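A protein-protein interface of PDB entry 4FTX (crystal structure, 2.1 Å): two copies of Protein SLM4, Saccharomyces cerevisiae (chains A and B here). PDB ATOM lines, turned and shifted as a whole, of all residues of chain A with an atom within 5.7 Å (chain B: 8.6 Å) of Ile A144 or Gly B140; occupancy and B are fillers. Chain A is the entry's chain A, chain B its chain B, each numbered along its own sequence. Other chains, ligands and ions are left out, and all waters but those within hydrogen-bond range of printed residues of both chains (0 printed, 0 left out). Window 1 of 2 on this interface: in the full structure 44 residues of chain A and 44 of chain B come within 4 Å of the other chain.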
ATOM      1  N   TYR A  96     -28.179  16.778 -14.943  1.00  0.00           N
ATOM      2  CA  TYR A  96     -27.241  15.820 -14.362  1.00  0.00           C
ATOM      3  C   TYR A  96     -26.039  16.552 -13.789  1.00  0.00           C
ATOM      4  O   TYR A  96     -25.279  17.179 -14.531  1.00  0.00           O
ATOM      5  CB  TYR A  96     -26.757  14.832 -15.426  1.00  0.00           C
ATOM      6  CG  TYR A  96     -27.867  14.004 -16.029  1.00  0.00           C
ATOM      7  CD1 TYR A  96     -28.541  13.050 -15.273  1.00  0.00           C
ATOM      8  CD2 TYR A  96     -28.237  14.175 -17.355  1.00  0.00           C
ATOM      9  CE1 TYR A  96     -29.559  12.302 -15.823  1.00  0.00           C
ATOM     10  CE2 TYR A  96     -29.241  13.423 -17.916  1.00  0.00           C
ATOM     11  CZ  TYR A  96     -29.904  12.490 -17.151  1.00  0.00           C
ATOM     12  OH  TYR A  96     -30.914  11.741 -17.712  1.00  0.00           O
ATOM     13  N   TYR A 139     -31.201  12.212 -26.572  1.00  0.00           N
ATOM     14  CA  TYR A 139     -30.649  13.033 -25.491  1.00  0.00           C
ATOM     15  C   TYR A 139     -29.577  12.293 -24.691  1.00  0.00           C
ATOM     16  O   TYR A 139     -28.599  12.892 -24.294  1.00  0.00           O
ATOM     17  CB  TYR A 139     -31.752  13.466 -24.526  1.00  0.00           C
ATOM     18  CG  TYR A 139     -32.630  14.582 -25.014  1.00  0.00           C
ATOM     19  CD1 TYR A 139     -32.116  15.867 -25.192  1.00  0.00           C
ATOM     20  CD2 TYR A 139     -33.985  14.369 -25.262  1.00  0.00           C
ATOM     21  CE1 TYR A 139     -32.922  16.907 -25.620  1.00  0.00           C
ATOM     22  CE2 TYR A 139     -34.803  15.403 -25.685  1.00  0.00           C
ATOM     23  CZ  TYR A 139     -34.257  16.673 -25.867  1.00  0.00           C
ATOM     24  OH  TYR A 139     -35.054  17.709 -26.292  1.00  0.00           O
ATOM     25  N   GLY A 140     -29.779  10.994 -24.445  1.00  0.00           N
ATOM     26  CA  GLY A 140     -28.798  10.196 -23.720  1.00  0.00           C
ATOM     27  C   GLY A 140     -27.413  10.259 -24.338  1.00  0.00           C
ATOM     28  O   GLY A 140     -26.389  10.321 -23.635  1.00  0.00           O
ATOM     29  N   LEU A 141     -27.385  10.267 -25.668  1.00  0.00           N
ATOM     30  CA  LEU A 141     -26.125  10.356 -26.403  1.00  0.00           C
ATOM     31  C   LEU A 141     -25.525  11.754 -26.326  1.00  0.00           C
ATOM     32  O   LEU A 141     -24.298  11.909 -26.297  1.00  0.00           O
ATOM     33  CB  LEU A 141     -26.312   9.922 -27.861  1.00  0.00           C
ATOM     34  CG  LEU A 141     -25.045   9.729 -28.690  1.00  0.00           C
ATOM     35  CD1 LEU A 141     -24.110   8.737 -28.014  1.00  0.00           C
ATOM     36  CD2 LEU A 141     -25.407   9.250 -30.088  1.00  0.00           C
ATOM     37  N   LEU A 142     -26.387  12.771 -26.292  1.00  0.00           N
ATOM     38  CA  LEU A 142     -25.902  14.162 -26.199  1.00  0.00           C
ATOM     39  C   LEU A 142     -25.230  14.353 -24.848  1.00  0.00           C
ATOM     40  O   LEU A 142     -24.181  14.969 -24.750  1.00  0.00           O
ATOM     41  CB  LEU A 142     -27.045  15.176 -26.369  1.00  0.00           C
ATOM     42  CG  LEU A 142     -27.538  15.450 -27.795  1.00  0.00           C
ATOM     43  CD1 LEU A 142     -28.861  16.204 -27.786  1.00  0.00           C
ATOM     44  CD2 LEU A 142     -26.496  16.224 -28.596  1.00  0.00           C
ATOM     45  N   VAL A 143     -25.844  13.785 -23.814  1.00  0.00           N
ATOM     46  CA  VAL A 143     -25.351  13.908 -22.442  1.00  0.00           C
ATOM     47  C   VAL A 143     -23.991  13.210 -22.260  1.00  0.00           C
ATOM     48  O   VAL A 143     -23.057  13.761 -21.646  1.00  0.00           O
ATOM     49  CB  VAL A 143     -26.420  13.365 -21.472  1.00  0.00           C
ATOM     50  CG1 VAL A 143     -25.850  13.157 -20.071  1.00  0.00           C
ATOM     51  CG2 VAL A 143     -27.619  14.313 -21.460  1.00  0.00           C
ATOM     52  N   ILE A 144     -23.875  12.005 -22.818  1.00  0.00           N
ATOM     53  CA  ILE A 144     -22.596  11.307 -22.807  1.00  0.00           C
ATOM     54  C   ILE A 144     -21.536  12.149 -23.517  1.00  0.00           C
ATOM     55  O   ILE A 144     -20.443  12.401 -22.987  1.00  0.00           O
ATOM     56  CB  ILE A 144     -22.716   9.925 -23.483  1.00  0.00           C
ATOM     57  CG1 ILE A 144     -23.552   8.976 -22.601  1.00  0.00           C
ATOM     58  CG2 ILE A 144     -21.348   9.338 -23.752  1.00  0.00           C
ATOM     59  CD1 ILE A 144     -23.935   7.684 -23.300  1.00  0.00           C
ATOM     60  N   LYS A 145     -21.887  12.589 -24.721  1.00  0.00           N
ATOM     61  CA  LYS A 145     -20.974  13.327 -25.578  1.00  0.00           C
ATOM     62  C   LYS A 145     -20.477  14.629 -24.942  1.00  0.00           C
ATOM     63  O   LYS A 145     -19.299  14.951 -25.032  1.00  0.00           O
ATOM     64  CB  LYS A 145     -21.660  13.631 -26.916  1.00  0.00           C
ATOM     65  CG  LYS A 145     -20.815  14.427 -27.890  1.00  0.00           C
ATOM     66  CD  LYS A 145     -21.588  14.708 -29.189  1.00  0.00           C
ATOM     67  CE  LYS A 145     -20.781  15.580 -30.132  1.00  0.00           C
ATOM     68  NZ  LYS A 145     -19.729  14.828 -30.875  1.00  0.00           N
ATOM     69  N   ILE A 146     -21.374  15.385 -24.318  1.00  0.00           N
ATOM     70  CA  ILE A 146     -20.987  16.698 -23.788  1.00  0.00           C
ATOM     71  C   ILE A 146     -20.142  16.518 -22.528  1.00  0.00           C
ATOM     72  O   ILE A 146     -19.230  17.293 -22.298  1.00  0.00           O
ATOM     73  CB  ILE A 146     -22.215  17.628 -23.521  1.00  0.00           C
ATOM     74  CG1 ILE A 146     -21.794  19.100 -23.515  1.00  0.00           C
ATOM     75  CG2 ILE A 146     -22.941  17.266 -22.218  1.00  0.00           C
ATOM     76  CD1 ILE A 146     -22.976  20.055 -23.654  1.00  0.00           C
ATOM     77  N   GLU A 147     -20.418  15.488 -21.726  1.00  0.00           N
ATOM     78  CA  GLU A 147     -19.548  15.230 -20.577  1.00  0.00           C
ATOM     79  C   GLU A 147     -18.118  14.933 -21.040  1.00  0.00           C
ATOM     80  O   GLU A 147     -17.141  15.523 -20.530  1.00  0.00           O
ATOM     81  CB  GLU A 147     -20.080  14.089 -19.698  1.00  0.00           C
ATOM     82  CG  GLU A 147     -19.241  13.903 -18.434  1.00  0.00           C
ATOM     83  CD  GLU A 147     -19.770  12.810 -17.534  1.00  0.00           C
ATOM     84  OE1 GLU A 147     -20.831  12.238 -17.851  1.00  0.00           O
ATOM     85  OE2 GLU A 147     -19.127  12.524 -16.505  1.00  0.00           O
ATOM     86  N   ARG A 148     -17.998  14.060 -22.041  1.00  0.00           N
ATOM     87  CA  ARG A 148     -16.673  13.735 -22.583  1.00  0.00           C
ATOM     88  C   ARG A 148     -15.993  14.961 -23.226  1.00  0.00           C
ATOM     89  O   ARG A 148     -14.810  15.204 -23.001  1.00  0.00           O
ATOM     90  CB  ARG A 148     -16.740  12.577 -23.586  1.00  0.00           C
ATOM     91  CG  ARG A 148     -17.414  11.314 -23.061  1.00  0.00           C
ATOM     92  CD  ARG A 148     -16.850  10.912 -21.714  1.00  0.00           C
ATOM     93  NE  ARG A 148     -17.596   9.807 -21.112  1.00  0.00           N
ATOM     94  CZ  ARG A 148     -17.156   8.554 -21.027  1.00  0.00           C
ATOM     95  NH1 ARG A 148     -15.961   8.217 -21.512  1.00  0.00           N
ATOM     96  NH2 ARG A 148     -17.913   7.634 -20.446  1.00  0.00           N
ATOM     97  N   ALA A 149     -16.743  15.722 -24.021  1.00  0.00           N
ATOM     98  CA  ALA A 149     -16.213  16.938 -24.654  1.00  0.00           C
ATOM     99  C   ALA A 149     -15.709  17.916 -23.601  1.00  0.00           C
ATOM    100  O   ALA A 149     -14.661  18.537 -23.768  1.00  0.00           O
ATOM    101  CB  ALA A 149     -17.291  17.616 -25.504  1.00  0.00           C
ATOM    102  N   TYR B  20     -20.610  10.799 -33.939  1.00  0.00           N
ATOM    103  CA  TYR B  20     -20.145  10.323 -32.646  1.00  0.00           C
ATOM    104  C   TYR B  20     -20.312   8.825 -32.533  1.00  0.00           C
ATOM    105  O   TYR B  20     -21.359   8.351 -32.094  1.00  0.00           O
ATOM    106  CB  TYR B  20     -20.953  10.981 -31.531  1.00  0.00           C
ATOM    107  CG  TYR B  20     -20.363  10.826 -30.153  1.00  0.00           C
ATOM    108  CD1 TYR B  20     -19.008  11.043 -29.927  1.00  0.00           C
ATOM    109  CD2 TYR B  20     -21.163  10.508 -29.067  1.00  0.00           C
ATOM    110  CE1 TYR B  20     -18.464  10.926 -28.661  1.00  0.00           C
ATOM    111  CE2 TYR B  20     -20.629  10.385 -27.797  1.00  0.00           C
ATOM    112  CZ  TYR B  20     -19.280  10.597 -27.600  1.00  0.00           C
ATOM    113  OH  TYR B  20     -18.735  10.482 -26.340  1.00  0.00           O
ATOM    114  N   ASP B  21     -19.285   8.080 -32.931  1.00  0.00           N
ATOM    115  CA  ASP B  21     -19.298   6.632 -32.754  1.00  0.00           C
ATOM    116  C   ASP B  21     -19.207   6.265 -31.269  1.00  0.00           C
ATOM    117  O   ASP B  21     -18.154   6.421 -30.642  1.00  0.00           O
ATOM    118  CB  ASP B  21     -18.179   5.961 -33.568  1.00  0.00           C
ATOM    119  CG  ASP B  21     -16.821   6.633 -33.379  1.00  0.00           C
ATOM    120  OD1 ASP B  21     -16.779   7.790 -32.902  1.00  0.00           O
ATOM    121  OD2 ASP B  21     -15.794   6.002 -33.716  1.00  0.00           O
ATOM    122  N   LEU B  22     -20.326   5.790 -30.713  1.00  0.00           N
ATOM    123  CA  LEU B  22     -20.377   5.285 -29.336  1.00  0.00           C
ATOM    124  C   LEU B  22     -19.338   4.165 -29.154  1.00  0.00           C
ATOM    125  O   LEU B  22     -19.055   3.728 -28.035  1.00  0.00           O
ATOM    126  CB  LEU B  22     -21.800   4.793 -29.006  1.00  0.00           C
ATOM    127  CG  LEU B  22     -22.266   4.498 -27.570  1.00  0.00           C
ATOM    128  CD1 LEU B  22     -22.244   5.731 -26.676  1.00  0.00           C
ATOM    129  CD2 LEU B  22     -23.659   3.887 -27.571  1.00  0.00           C
ATOM    130  N   VAL B  25     -16.066   5.246 -27.345  1.00  0.00           N
ATOM    131  CA  VAL B  25     -16.341   5.722 -25.987  1.00  0.00           C
ATOM    132  C   VAL B  25     -16.154   4.630 -24.934  1.00  0.00           C
ATOM    133  O   VAL B  25     -16.850   3.611 -24.951  1.00  0.00           O
ATOM    134  CB  VAL B  25     -17.772   6.274 -25.852  1.00  0.00           C
ATOM    135  CG1 VAL B  25     -17.928   6.991 -24.525  1.00  0.00           C
ATOM    136  CG2 VAL B  25     -18.111   7.213 -27.005  1.00  0.00           C
ATOM    137  N   ASP B  26     -15.222   4.853 -24.011  1.00  0.00           N
ATOM    138  CA  ASP B  26     -14.977   3.902 -22.933  1.00  0.00           C
ATOM    139  C   ASP B  26     -15.763   4.266 -21.690  1.00  0.00           C
ATOM    140  O   ASP B  26     -15.807   5.428 -21.290  1.00  0.00           O
ATOM    141  CB  ASP B  26     -13.489   3.812 -22.603  1.00  0.00           C
ATOM    142  CG  ASP B  26     -12.750   2.860 -23.519  1.00  0.00           C
ATOM    143  OD1 ASP B  26     -12.952   1.632 -23.385  1.00  0.00           O
ATOM    144  OD2 ASP B  26     -11.966   3.336 -24.369  1.00  0.00           O
ATOM    145  N   PHE B  27     -16.390   3.264 -21.090  1.00  0.00           N
ATOM    146  CA  PHE B  27     -17.175   3.454 -19.881  1.00  0.00           C
ATOM    147  C   PHE B  27     -16.552   2.648 -18.759  1.00  0.00           C
ATOM    148  O   PHE B  27     -16.013   1.569 -18.997  1.00  0.00           O
ATOM    149  CB  PHE B  27     -18.619   3.023 -20.111  1.00  0.00           C
ATOM    150  CG  PHE B  27     -19.340   3.855 -21.126  1.00  0.00           C
ATOM    151  CD1 PHE B  27     -19.762   5.141 -20.813  1.00  0.00           C
ATOM    152  CD2 PHE B  27     -19.596   3.358 -22.401  1.00  0.00           C
ATOM    153  CE1 PHE B  27     -20.422   5.925 -21.755  1.00  0.00           C
ATOM    154  CE2 PHE B  27     -20.261   4.132 -23.345  1.00  0.00           C
ATOM    155  CZ  PHE B  27     -20.677   5.417 -23.020  1.00  0.00           C
ATOM    156  N   SER B  94     -34.261  13.367 -14.823  1.00  0.00           N
ATOM    157  CA  SER B  94     -34.630  13.520 -16.220  1.00  0.00           C
ATOM    158  C   SER B  94     -35.976  12.925 -16.508  1.00  0.00           C
ATOM    159  O   SER B  94     -36.388  11.942 -15.874  1.00  0.00           O
ATOM    160  CB  SER B  94     -33.583  12.869 -17.136  1.00  0.00           C
ATOM    161  OG  SER B  94     -33.334  11.525 -16.746  1.00  0.00           O
ATOM    162  N   TYR B  96     -37.612  12.074 -20.160  1.00  0.00           N
ATOM    163  CA  TYR B  96     -37.553  12.124 -21.612  1.00  0.00           C
ATOM    164  C   TYR B  96     -38.779  11.430 -22.205  1.00  0.00           C
ATOM    165  O   TYR B  96     -38.987  10.235 -21.987  1.00  0.00           O
ATOM    166  CB  TYR B  96     -36.293  11.456 -22.140  1.00  0.00           C
ATOM    167  CG  TYR B  96     -34.976  12.048 -21.674  1.00  0.00           C
ATOM    168  CD1 TYR B  96     -34.625  13.374 -21.960  1.00  0.00           C
ATOM    169  CD2 TYR B  96     -34.054  11.261 -21.005  1.00  0.00           C
ATOM    170  CE1 TYR B  96     -33.396  13.898 -21.543  1.00  0.00           C
ATOM    171  CE2 TYR B  96     -32.836  11.763 -20.593  1.00  0.00           C
ATOM    172  CZ  TYR B  96     -32.499  13.076 -20.865  1.00  0.00           C
ATOM    173  OH  TYR B  96     -31.269  13.555 -20.445  1.00  0.00           O
ATOM    174  N   ILE B 107     -39.090   8.337 -19.829  1.00  0.00           N
ATOM    175  CA  ILE B 107     -37.941   7.784 -19.159  1.00  0.00           C
ATOM    176  C   ILE B 107     -37.488   8.707 -18.032  1.00  0.00           C
ATOM    177  O   ILE B 107     -37.089   9.864 -18.256  1.00  0.00           O
ATOM    178  CB  ILE B 107     -36.776   7.562 -20.146  1.00  0.00           C
ATOM    179  CG1 ILE B 107     -37.174   6.572 -21.250  1.00  0.00           C
ATOM    180  CG2 ILE B 107     -35.537   7.075 -19.400  1.00  0.00           C
ATOM    181  CD1 ILE B 107     -36.125   6.458 -22.363  1.00  0.00           C
ATOM    182  N   THR B 109     -35.025   9.118 -14.378  1.00  0.00           N
ATOM    183  CA  THR B 109     -33.777   8.683 -13.765  1.00  0.00           C
ATOM    184  C   THR B 109     -33.748   9.132 -12.322  1.00  0.00           C
ATOM    185  O   THR B 109     -34.172  10.237 -11.992  1.00  0.00           O
ATOM    186  CB  THR B 109     -32.519   9.216 -14.500  1.00  0.00           C
ATOM    187  OG1 THR B 109     -32.624  10.635 -14.705  1.00  0.00           O
ATOM    188  CG2 THR B 109     -32.349   8.513 -15.852  1.00  0.00           C
ATOM    189  N   HIS B 116     -27.232   4.583  -9.771  1.00  0.00           N
ATOM    190  CA  HIS B 116     -27.994   5.222 -10.828  1.00  0.00           C
ATOM    191  C   HIS B 116     -29.108   4.299 -11.244  1.00  0.00           C
ATOM    192  O   HIS B 116     -28.861   3.157 -11.638  1.00  0.00           O
ATOM    193  CB  HIS B 116     -27.107   5.504 -12.038  1.00  0.00           C
ATOM    194  CG  HIS B 116     -26.132   6.617 -11.828  1.00  0.00           C
ATOM    195  ND1 HIS B 116     -25.208   6.972 -12.768  1.00  0.00           N
ATOM    196  CD2 HIS B 116     -25.939   7.464 -10.763  1.00  0.00           C
ATOM    197  CE1 HIS B 116     -24.484   7.989 -12.313  1.00  0.00           C
ATOM    198  NE2 HIS B 116     -24.920   8.300 -11.093  1.00  0.00           N
ATOM    199  N   CYS B 118     -32.899   3.914 -13.535  1.00  0.00           N
ATOM    200  CA  CYS B 118     -33.633   4.405 -14.697  1.00  0.00           C
ATOM    201  C   CYS B 118     -34.928   3.618 -14.812  1.00  0.00           C
ATOM    202  O   CYS B 118     -34.919   2.390 -14.741  1.00  0.00           O
ATOM    203  CB  CYS B 118     -32.802   4.184 -15.959  1.00  0.00           C
ATOM    204  SG  CYS B 118     -33.504   4.928 -17.447  1.00  0.00           S
ATOM    205  N   PHE B 137     -22.060   4.032 -14.026  1.00  0.00           N
ATOM    206  CA  PHE B 137     -22.826   3.767 -15.251  1.00  0.00           C
ATOM    207  C   PHE B 137     -23.567   5.053 -15.590  1.00  0.00           C
ATOM    208  O   PHE B 137     -24.492   5.427 -14.885  1.00  0.00           O
ATOM    209  CB  PHE B 137     -23.817   2.626 -14.982  1.00  0.00           C
ATOM    210  CG  PHE B 137     -24.441   1.998 -16.212  1.00  0.00           C
ATOM    211  CD1 PHE B 137     -25.029   2.768 -17.212  1.00  0.00           C
ATOM    212  CD2 PHE B 137     -24.508   0.607 -16.323  1.00  0.00           C
ATOM    213  CE1 PHE B 137     -25.643   2.158 -18.320  1.00  0.00           C
ATOM    214  CE2 PHE B 137     -25.118  -0.006 -17.423  1.00  0.00           C
ATOM    215  CZ  PHE B 137     -25.691   0.773 -18.423  1.00  0.00           C
ATOM    216  N   PRO B 138     -23.145   5.744 -16.668  1.00  0.00           N
ATOM    217  CA  PRO B 138     -23.697   7.071 -16.964  1.00  0.00           C
ATOM    218  C   PRO B 138     -25.195   7.010 -17.237  1.00  0.00           C
ATOM    219  O   PRO B 138     -25.678   6.050 -17.854  1.00  0.00           O
ATOM    220  CB  PRO B 138     -22.935   7.511 -18.223  1.00  0.00           C
ATOM    221  CG  PRO B 138     -21.767   6.586 -18.328  1.00  0.00           C
ATOM    222  CD  PRO B 138     -22.183   5.300 -17.693  1.00  0.00           C
ATOM    223  N   TYR B 139     -25.921   8.013 -16.758  1.00  0.00           N
ATOM    224  CA  TYR B 139     -27.355   8.074 -16.970  1.00  0.00           C
ATOM    225  C   TYR B 139     -27.718   8.104 -18.451  1.00  0.00           C
ATOM    226  O   TYR B 139     -28.731   7.539 -18.845  1.00  0.00           O
ATOM    227  CB  TYR B 139     -27.962   9.303 -16.282  1.00  0.00           C
ATOM    228  CG  TYR B 139     -28.160   9.205 -14.777  1.00  0.00           C
ATOM    229  CD1 TYR B 139     -29.030   8.276 -14.233  1.00  0.00           C
ATOM    230  CD2 TYR B 139     -27.496  10.071 -13.904  1.00  0.00           C
ATOM    231  CE1 TYR B 139     -29.234   8.189 -12.863  1.00  0.00           C
ATOM    232  CE2 TYR B 139     -27.693  10.003 -12.527  1.00  0.00           C
ATOM    233  CZ  TYR B 139     -28.572   9.055 -12.017  1.00  0.00           C
ATOM    234  OH  TYR B 139     -28.786   8.957 -10.666  1.00  0.00           O
ATOM    235  N   GLY B 140     -26.902   8.793 -19.259  1.00  0.00           N
ATOM    236  CA  GLY B 140     -27.140   8.895 -20.689  1.00  0.00           C
ATOM    237  C   GLY B 140     -27.206   7.523 -21.349  1.00  0.00           C
ATOM    238  O   GLY B 140     -28.041   7.278 -22.228  1.00  0.00           O
ATOM    239  N   LEU B 141     -26.321   6.628 -20.904  1.00  0.00           N
ATOM    240  CA  LEU B 141     -26.283   5.249 -21.394  1.00  0.00           C
ATOM    241  C   LEU B 141     -27.497   4.474 -20.930  1.00  0.00           C
ATOM    242  O   LEU B 141     -28.073   3.711 -21.702  1.00  0.00           O
ATOM    243  CB  LEU B 141     -24.999   4.531 -20.958  1.00  0.00           C
ATOM    244  CG  LEU B 141     -24.664   3.188 -21.624  1.00  0.00           C
ATOM    245  CD1 LEU B 141     -24.697   3.297 -23.143  1.00  0.00           C
ATOM    246  CD2 LEU B 141     -23.293   2.717 -21.170  1.00  0.00           C
ATOM    247  N   LEU B 142     -27.896   4.675 -19.678  1.00  0.00           N
ATOM    248  CA  LEU B 142     -29.089   3.997 -19.156  1.00  0.00           C
ATOM    249  C   LEU B 142     -30.340   4.380 -19.931  1.00  0.00           C
ATOM    250  O   LEU B 142     -31.190   3.538 -20.199  1.00  0.00           O
ATOM    251  CB  LEU B 142     -29.298   4.301 -17.681  1.00  0.00           C
ATOM    252  CG  LEU B 142     -28.432   3.574 -16.656  1.00  0.00           C
ATOM    253  CD1 LEU B 142     -28.633   4.212 -15.285  1.00  0.00           C
ATOM    254  CD2 LEU B 142     -28.787   2.075 -16.606  1.00  0.00           C
ATOM    255  N   VAL B 143     -30.429   5.654 -20.307  1.00  0.00           N
ATOM    256  CA  VAL B 143     -31.574   6.172 -21.048  1.00  0.00           C
ATOM    257  C   VAL B 143     -31.648   5.574 -22.460  1.00  0.00           C
ATOM    258  O   VAL B 143     -32.725   5.131 -22.914  1.00  0.00           O
ATOM    259  CB  VAL B 143     -31.486   7.715 -21.109  1.00  0.00           C
ATOM    260  CG1 VAL B 143     -32.438   8.289 -22.155  1.00  0.00           C
ATOM    261  CG2 VAL B 143     -31.749   8.293 -19.723  1.00  0.00           C
ATOM    262  N   ILE B 144     -30.508   5.579 -23.157  1.00  0.00           N
ATOM    263  CA  ILE B 144     -30.412   4.886 -24.449  1.00  0.00           C
ATOM    264  C   ILE B 144     -30.854   3.417 -24.282  1.00  0.00           C
ATOM    265  O   ILE B 144     -31.742   2.920 -25.003  1.00  0.00           O
ATOM    266  CB  ILE B 144     -28.979   4.967 -25.024  1.00  0.00           C
ATOM    267  CG1 ILE B 144     -28.635   6.419 -25.401  1.00  0.00           C
ATOM    268  CG2 ILE B 144     -28.803   4.050 -26.245  1.00  0.00           C
ATOM    269  CD1 ILE B 144     -27.193   6.638 -25.748  1.00  0.00           C
ATOM    270  N   LYS B 145     -30.269   2.755 -23.286  1.00  0.00           N
ATOM    271  CA  LYS B 145     -30.481   1.319 -23.065  1.00  0.00           C
ATOM    272  C   LYS B 145     -31.943   0.988 -22.826  1.00  0.00           C
ATOM    273  O   LYS B 145     -32.485   0.038 -23.406  1.00  0.00           O
ATOM    274  CB  LYS B 145     -29.637   0.828 -21.888  1.00  0.00           C
ATOM    275  CG  LYS B 145     -29.623  -0.689 -21.732  1.00  0.00           C
ATOM    276  CD  LYS B 145     -28.817  -1.101 -20.503  1.00  0.00           C
ATOM    277  CE  LYS B 145     -29.039  -2.582 -20.227  1.00  0.00           C
ATOM    278  NZ  LYS B 145     -28.292  -3.419 -21.207  1.00  0.00           N
ATOM    279  N   ILE B 146     -32.594   1.776 -21.980  1.00  0.00           N
ATOM    280  CA  ILE B 146     -33.961   1.446 -21.602  1.00  0.00           C
ATOM    281  C   ILE B 146     -34.924   1.695 -22.760  1.00  0.00           C
ATOM    282  O   ILE B 146     -35.888   0.955 -22.923  1.00  0.00           O
ATOM    283  CB  ILE B 146     -34.412   2.144 -20.301  1.00  0.00           C
ATOM    284  CG1 ILE B 146     -35.515   1.327 -19.621  1.00  0.00           C
ATOM    285  CG2 ILE B 146     -34.829   3.601 -20.565  1.00  0.00           C
ATOM    286  CD1 ILE B 146     -35.750   1.707 -18.169  1.00  0.00           C
ATOM    287  N   GLU B 147     -34.655   2.718 -23.571  1.00  0.00           N
ATOM    288  CA  GLU B 147     -35.503   2.965 -24.723  1.00  0.00           C
ATOM    289  C   GLU B 147     -35.404   1.820 -25.729  1.00  0.00           C
ATOM    290  O   GLU B 147     -36.420   1.379 -26.248  1.00  0.00           O
ATOM    291  CB  GLU B 147     -35.176   4.303 -25.418  1.00  0.00           C
ATOM    292  CG  GLU B 147     -36.098   4.576 -26.617  1.00  0.00           C
ATOM    293  CD  GLU B 147     -35.816   5.906 -27.320  1.00  0.00           C
ATOM    294  OE1 GLU B 147     -34.953   6.672 -26.842  1.00  0.00           O
ATOM    295  OE2 GLU B 147     -36.456   6.183 -28.361  1.00  0.00           O
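OH of Tyr A96 is in hydrogen-bond range of OG of Ser B94 (2.6 Å). The side-chain hydroxyl (OH) of Tyr A96 sits close to the side-chain hydroxyl (OH) of Tyr B96 (3.3 Å). The guanidinium group of Arg A148 lies within hydrogen-bond range of the backbone carbonyl oxygen of Asp B26 (2.8 Å).
The side-chain hydroxyl (OG1) of Thr B109 is in hydrogen-bond range of the backbone NH (N) of Ser B94, 3.2 Å away. N of Ile B107 sits at hydrogen-bond distance from O of Tyr B96, 2.9 Å away.
Among the printed residues, merely in contact across the chains: Arg A148 with Phe B27 (3.1 Å), Gly A140 with Gly B140 (3.4 Å), Tyr A96 with Tyr B139 (3.4 Å), Tyr A139 with Tyr B96 (3.4 Å), Lys A145 with Tyr B20 (3.5 Å), Ile A144 with Leu B141 (3.5 Å), Leu A141 with Tyr B20 (3.6 Å), Arg A148 with Tyr B20 (3.6 Å), Tyr A96 with Thr B109 (3.6 Å), Leu A141 with Ile B144 (3.6 Å), Leu A141 with Leu B22 (3.8 Å), Arg A148 with Val B25 (3.8 Å), Ile A144 with Gly B140 (3.8 Å), Ile A144 with Tyr B20 (3.9 Å), Val A143 with Tyr B96 (3.9 Å), Gly A140 with Ile B144 (3.9 Å) and Ile A144 with Phe B27 (3.98 Å).
Printed residues of chain B within 4 Å of Ile A144: Tyr B20 (3.9 Å), Phe B27 (3.98 Å), Gly B140 (3.8 Å) and Leu B141 (3.5 Å). Gly B140 touches just these residues of chain A: Gly A140 and Ile A144. Of the printed residues of chain A, Leu B22 touches Leu A141. Of the printed residues of chain B, Val A143 touches Tyr B96 (3.9 Å). Ile B146 touches none of the printed residues of chain A. The nearest printed residue of chain B that does not touch Ile A144 is Ile B144 (4.2 Å). The nearest residue of chain A that does not touch Gly B140 is Val A143 (4.5 Å). The nearest printed residue of chain B that does not touch Leu A141 is Gly B140 (4.6 Å).
Of the 23 printed residues of chain B, 12 touch a printed residue of chain A. Hydrophobic or aromatic side chains of chain B within 4 Å of the printed part of chain A: Tyr B20, Leu B22, Val B25, Phe B27, Tyr B96, Tyr B139 and Ile B144. Of the 12 printed residues of chain A, 8 touch a printed residue of chain B. Hydrophobic or aromatic side chains of chain A that line the printed part of chain B: Tyr A96, Tyr A139, Leu A141, Val A143 and Ile A144. Along chain A the printed residues that touch a printed residue of chain B span positions 96 to 148. Among the printed residues, 20 pairs touch across the chains.
Gly A140 touches its own counterpart, Gly B140. Gly A140 touches Ile B144, and with the chains exchanged Ile A144 touches Gly B140. Leu A141 touches Ile B144, and with the chains exchanged Ile A144 touches Leu B141. Val A143 touches Tyr B96, but with the chains exchanged Tyr A96 does not touch Val B143 (4.1 Å).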
